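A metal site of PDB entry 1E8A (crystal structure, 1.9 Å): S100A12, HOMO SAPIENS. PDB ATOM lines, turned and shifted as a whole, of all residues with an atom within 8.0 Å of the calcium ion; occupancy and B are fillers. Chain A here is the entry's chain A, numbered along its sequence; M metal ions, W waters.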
ATOM      1  N   THR A  26     -14.067  24.787  23.683  1.00  0.00           N
ATOM      2  CA  THR A  26     -14.309  23.667  24.565  1.00  0.00           C
ATOM      3  C   THR A  26     -13.323  23.670  25.727  1.00  0.00           C
ATOM      4  O   THR A  26     -12.236  24.196  25.624  1.00  0.00           O
ATOM      5  CB  THR A  26     -14.302  22.305  23.871  1.00  0.00           C
ATOM      6  OG1 THR A  26     -12.983  21.960  23.462  1.00  0.00           O
ATOM      7  CG2 THR A  26     -15.076  22.290  22.563  1.00  0.00           C
ATOM      8  N   LEU A  27     -13.754  23.092  26.829  1.00  0.00           N
ATOM      9  CA  LEU A  27     -12.976  22.982  28.069  1.00  0.00           C
ATOM     10  C   LEU A  27     -12.310  21.645  28.139  1.00  0.00           C
ATOM     11  O   LEU A  27     -12.965  20.592  28.097  1.00  0.00           O
ATOM     12  CB  LEU A  27     -13.880  23.138  29.301  1.00  0.00           C
ATOM     13  CG  LEU A  27     -14.606  24.465  29.433  1.00  0.00           C
ATOM     14  CD1 LEU A  27     -15.757  24.318  30.409  1.00  0.00           C
ATOM     15  CD2 LEU A  27     -13.692  25.563  29.914  1.00  0.00           C
ATOM     16  N   PHE A  57     -16.321  16.080  35.718  1.00  0.00           N
ATOM     17  CA  PHE A  57     -15.939  16.140  34.302  1.00  0.00           C
ATOM     18  C   PHE A  57     -16.526  15.005  33.503  1.00  0.00           C
ATOM     19  O   PHE A  57     -17.013  15.220  32.384  1.00  0.00           O
ATOM     20  CB  PHE A  57     -14.430  16.136  34.127  1.00  0.00           C
ATOM     21  CG  PHE A  57     -13.997  16.162  32.688  1.00  0.00           C
ATOM     22  CD1 PHE A  57     -13.799  15.002  31.993  1.00  0.00           C
ATOM     23  CD2 PHE A  57     -13.734  17.359  32.042  1.00  0.00           C
ATOM     24  CE1 PHE A  57     -13.340  15.029  30.655  1.00  0.00           C
ATOM     25  CE2 PHE A  57     -13.335  17.378  30.716  1.00  0.00           C
ATOM     26  CZ  PHE A  57     -13.162  16.219  30.037  1.00  0.00           C
ATOM     27  N   GLN A  58     -16.476  13.822  34.088  1.00  0.00           N
ATOM     28  CA  GLN A  58     -17.004  12.648  33.460  1.00  0.00           C
ATOM     29  C   GLN A  58     -18.501  12.788  33.238  1.00  0.00           C
ATOM     30  O   GLN A  58     -18.993  12.510  32.144  1.00  0.00           O
ATOM     31  CB  GLN A  58     -16.704  11.432  34.314  1.00  0.00           C
ATOM     32  CG  GLN A  58     -15.272  10.986  34.125  1.00  0.00           C
ATOM     33  CD  GLN A  58     -14.985  10.658  32.666  1.00  0.00           C
ATOM     34  OE1 GLN A  58     -15.794  10.030  31.973  1.00  0.00           O
ATOM     35  NE2 GLN A  58     -13.822  11.065  32.199  1.00  0.00           N
ATOM     36  N   LEU A  60     -20.166  15.497  32.895  1.00  0.00           N
ATOM     37  CA  LEU A  60     -20.393  16.523  31.845  1.00  0.00           C
ATOM     38  C   LEU A  60     -20.043  16.051  30.429  1.00  0.00           C
ATOM     39  O   LEU A  60     -20.687  16.435  29.474  1.00  0.00           O
ATOM     40  CB  LEU A  60     -19.622  17.812  32.116  1.00  0.00           C
ATOM     41  CG  LEU A  60     -19.983  18.616  33.391  1.00  0.00           C
ATOM     42  CD1 LEU A  60     -19.114  19.839  33.626  1.00  0.00           C
ATOM     43  CD2 LEU A  60     -21.456  18.953  33.413  1.00  0.00           C
ATOM     44  N   ASP A  61     -19.012  15.233  30.303  1.00  0.00           N
ATOM     45  CA  ASP A  61     -18.535  14.828  29.008  1.00  0.00           C
ATOM     46  C   ASP A  61     -19.368  13.689  28.427  1.00  0.00           C
ATOM     47  O   ASP A  61     -18.908  12.556  28.293  1.00  0.00           O
ATOM     48  CB  ASP A  61     -17.056  14.448  29.148  1.00  0.00           C
ATOM     49  CG  ASP A  61     -16.383  14.146  27.808  1.00  0.00           C
ATOM     50  OD1 ASP A  61     -16.959  14.484  26.753  1.00  0.00           O
ATOM     51  OD2 ASP A  61     -15.244  13.595  27.741  1.00  0.00           O
ATOM     52  N   ALA A  62     -20.559  14.028  27.984  1.00  0.00           N
ATOM     53  CA  ALA A  62     -21.543  13.085  27.497  1.00  0.00           C
ATOM     54  C   ALA A  62     -21.131  12.303  26.258  1.00  0.00           C
ATOM     55  O   ALA A  62     -21.527  11.169  26.129  1.00  0.00           O
ATOM     56  CB  ALA A  62     -22.929  13.759  27.269  1.00  0.00           C
ATOM     57  N   ASN A  63     -20.279  12.857  25.402  1.00  0.00           N
ATOM     58  CA  ASN A  63     -19.839  12.141  24.212  1.00  0.00           C
ATOM     59  C   ASN A  63     -18.424  11.590  24.357  1.00  0.00           C
ATOM     60  O   ASN A  63     -17.799  11.097  23.403  1.00  0.00           O
ATOM     61  CB  ASN A  63     -20.001  12.993  22.971  1.00  0.00           C
ATOM     62  CG  ASN A  63     -18.997  14.119  22.890  1.00  0.00           C
ATOM     63  OD1 ASN A  63     -18.363  14.522  23.847  1.00  0.00           O
ATOM     64  ND2 ASN A  63     -18.888  14.666  21.704  1.00  0.00           N
ATOM     65  N   GLN A  64     -17.935  11.704  25.593  1.00  0.00           N
ATOM     66  CA  GLN A  64     -16.712  11.098  26.056  1.00  0.00           C
ATOM     67  C   GLN A  64     -15.542  11.408  25.111  1.00  0.00           C
ATOM     68  O   GLN A  64     -14.734  10.530  24.790  1.00  0.00           O
ATOM     69  CB  GLN A  64     -16.903   9.613  26.207  1.00  0.00           C
ATOM     70  CG  GLN A  64     -17.815   9.212  27.366  1.00  0.00           C
ATOM     71  CD  GLN A  64     -17.110   9.346  28.701  1.00  0.00           C
ATOM     72  OE1 GLN A  64     -16.344   8.460  29.062  1.00  0.00           O
ATOM     73  NE2 GLN A  64     -17.333  10.445  29.419  1.00  0.00           N
ATOM     74  N   ASP A  65     -15.473  12.642  24.660  1.00  0.00           N
ATOM     75  CA  ASP A  65     -14.419  13.023  23.746  1.00  0.00           C
ATOM     76  C   ASP A  65     -13.306  13.846  24.493  1.00  0.00           C
ATOM     77  O   ASP A  65     -12.406  14.394  23.883  1.00  0.00           O
ATOM     78  CB  ASP A  65     -14.988  13.780  22.581  1.00  0.00           C
ATOM     79  CG  ASP A  65     -15.472  15.172  22.963  1.00  0.00           C
ATOM     80  OD1 ASP A  65     -15.532  15.527  24.183  1.00  0.00           O
ATOM     81  OD2 ASP A  65     -15.815  15.988  22.100  1.00  0.00           O
ATOM     82  N   GLU A  66     -13.362  13.840  25.808  1.00  0.00           N
ATOM     83  CA  GLU A  66     -12.368  14.479  26.660  1.00  0.00           C
ATOM     84  C   GLU A  66     -12.358  16.013  26.630  1.00  0.00           C
ATOM     85  O   GLU A  66     -11.404  16.627  27.101  1.00  0.00           O
ATOM     86  CB  GLU A  66     -10.966  13.891  26.464  1.00  0.00           C
ATOM     87  CG  GLU A  66     -10.927  12.478  27.030  1.00  0.00           C
ATOM     88  CD  GLU A  66      -9.578  11.847  26.899  1.00  0.00           C
ATOM     89  OE1 GLU A  66      -8.636  12.519  26.430  1.00  0.00           O
ATOM     90  OE2 GLU A  66      -9.452  10.656  27.280  1.00  0.00           O
ATOM     91  N   GLN A  67     -13.453  16.587  26.180  1.00  0.00           N
ATOM     92  CA  GLN A  67     -13.652  18.040  26.228  1.00  0.00           C
ATOM     93  C   GLN A  67     -15.042  18.270  26.689  1.00  0.00           C
ATOM     94  O   GLN A  67     -15.934  17.439  26.420  1.00  0.00           O
ATOM     95  CB  GLN A  67     -13.606  18.621  24.840  1.00  0.00           C
ATOM     96  CG  GLN A  67     -12.316  18.372  24.175  1.00  0.00           C
ATOM     97  CD  GLN A  67     -11.244  19.277  24.732  1.00  0.00           C
ATOM     98  OE1 GLN A  67     -11.513  20.457  25.005  1.00  0.00           O
ATOM     99  NE2 GLN A  67     -10.048  18.764  24.888  1.00  0.00           N
ATOM    100  N   VAL A  68     -15.250  19.388  27.373  1.00  0.00           N
ATOM    101  CA  VAL A  68     -16.568  19.831  27.691  1.00  0.00           C
ATOM    102  C   VAL A  68     -16.963  21.017  26.837  1.00  0.00           C
ATOM    103  O   VAL A  68     -16.408  22.134  26.958  1.00  0.00           O
ATOM    104  CB  VAL A  68     -16.731  20.083  29.206  1.00  0.00           C
ATOM    105  CG1 VAL A  68     -18.112  20.625  29.472  1.00  0.00           C
ATOM    106  CG2 VAL A  68     -16.442  18.780  30.042  1.00  0.00           C
ATOM    107  N   ASP A  69     -17.871  20.748  25.883  1.00  0.00           N
ATOM    108  CA  ASP A  69     -18.331  21.797  24.993  1.00  0.00           C
ATOM    109  C   ASP A  69     -19.459  22.636  25.645  1.00  0.00           C
ATOM    110  O   ASP A  69     -19.865  22.364  26.800  1.00  0.00           O
ATOM    111  CB  ASP A  69     -18.775  21.228  23.644  1.00  0.00           C
ATOM    112  CG  ASP A  69     -19.959  20.362  23.721  1.00  0.00           C
ATOM    113  OD1 ASP A  69     -20.842  20.573  24.592  1.00  0.00           O
ATOM    114  OD2 ASP A  69     -20.107  19.446  22.868  1.00  0.00           O
ATOM    115  N   PHE A  70     -19.903  23.669  24.954  1.00  0.00           N
ATOM    116  CA  PHE A  70     -20.758  24.643  25.587  1.00  0.00           C
ATOM    117  C   PHE A  70     -22.059  23.980  25.996  1.00  0.00           C
ATOM    118  O   PHE A  70     -22.560  24.184  27.079  1.00  0.00           O
ATOM    119  CB  PHE A  70     -21.004  25.953  24.758  1.00  0.00           C
ATOM    120  CG  PHE A  70     -21.762  26.975  25.523  1.00  0.00           C
ATOM    121  CD1 PHE A  70     -21.141  27.676  26.582  1.00  0.00           C
ATOM    122  CD2 PHE A  70     -23.115  27.108  25.362  1.00  0.00           C
ATOM    123  CE1 PHE A  70     -21.858  28.536  27.370  1.00  0.00           C
ATOM    124  CE2 PHE A  70     -23.834  28.034  26.153  1.00  0.00           C
ATOM    125  CZ  PHE A  70     -23.219  28.723  27.140  1.00  0.00           C
ATOM    126  N   GLU A  72     -22.587  20.829  26.660  1.00  0.00           N
ATOM    127  CA  GLU A  72     -22.349  20.035  27.847  1.00  0.00           C
ATOM    128  C   GLU A  72     -22.204  20.890  29.109  1.00  0.00           C
ATOM    129  O   GLU A  72     -22.697  20.531  30.167  1.00  0.00           O
ATOM    130  CB  GLU A  72     -21.109  19.155  27.641  1.00  0.00           C
ATOM    131  CG  GLU A  72     -21.337  18.066  26.611  1.00  0.00           C
ATOM    132  CD  GLU A  72     -20.047  17.359  26.184  1.00  0.00           C
ATOM    133  OE1 GLU A  72     -18.992  18.001  26.359  1.00  0.00           O
ATOM    134  OE2 GLU A  72     -20.099  16.205  25.694  1.00  0.00           O
ATOM    135  N   PHE A  73     -21.521  22.026  28.984  1.00  0.00           N
ATOM    136  CA  PHE A  73     -21.298  22.929  30.099  1.00  0.00           C
ATOM    137  C   PHE A  73     -22.643  23.454  30.642  1.00  0.00           C
ATOM    138  O   PHE A  73     -22.759  23.781  31.838  1.00  0.00           O
ATOM    139  CB  PHE A  73     -20.387  24.083  29.643  1.00  0.00           C
ATOM    140  CG  PHE A  73     -20.231  25.177  30.626  1.00  0.00           C
ATOM    141  CD1 PHE A  73     -19.290  25.112  31.598  1.00  0.00           C
ATOM    142  CD2 PHE A  73     -20.996  26.319  30.540  1.00  0.00           C
ATOM    143  CE1 PHE A  73     -19.098  26.128  32.483  1.00  0.00           C
ATOM    144  CE2 PHE A  73     -20.783  27.353  31.445  1.00  0.00           C
ATOM    145  CZ  PHE A  73     -19.864  27.239  32.406  1.00  0.00           C
HETATM  146 CA    CA M   1     -17.565  16.222  25.243  1.00  0.00          CA
HETATM  147  O   HOH W   1     -17.831  17.542  23.338  1.00  0.00           O
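The side-chain amide oxygen of Gln 67 lies close to the backbone carbonyl oxygen of Leu 27 (3.4 Å). OE1 of Gln 67 is in hydrogen-bond range of OG1 of Thr 26 (2.6 Å). O of Asp 61 lies within hydrogen-bond range of NE2 of Gln 64 (2.9 Å). The side-chain carboxylate (OD2) of Asp 61 sits at hydrogen-bond distance from the backbone NH (N) of Glu 66. OD1 of Asp 69 is in hydrogen-bond range of N of Glu 72. The backbone NH (N) of Ala 62 sits close to the side-chain carboxylate (OE2) of Glu 72, at 3.2 Å.
Of the 17 residues printed, 5 come within 4 Å of the calcium ion.
The calcium ion is bound by water W1 (2.3 Å), the side-chain amide oxygen (OD1) of Asn 63 (2.3 Å), the backbone carbonyl oxygen (O) of Gln 67 (2.4 Å), the side-chain carboxylate (OD1) of Asp 61 (2.4 Å), the side-chain carboxylate (OD1) of Asp 65 (2.4 Å), the side-chain carboxylate (OE1) of Glu 72 (2.5 Å) and the side-chain carboxylate (OE2) of Glu 72 (2.6 Å). The calcium ion has seven donor atoms within binding distance.
Water W1 lies within hydrogen-bond range of OD2 of Asp 65 (2.8 Å), OD2 of Asp 69 (3.0 Å) and ND2 of Asn 63 (3.5 Å).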
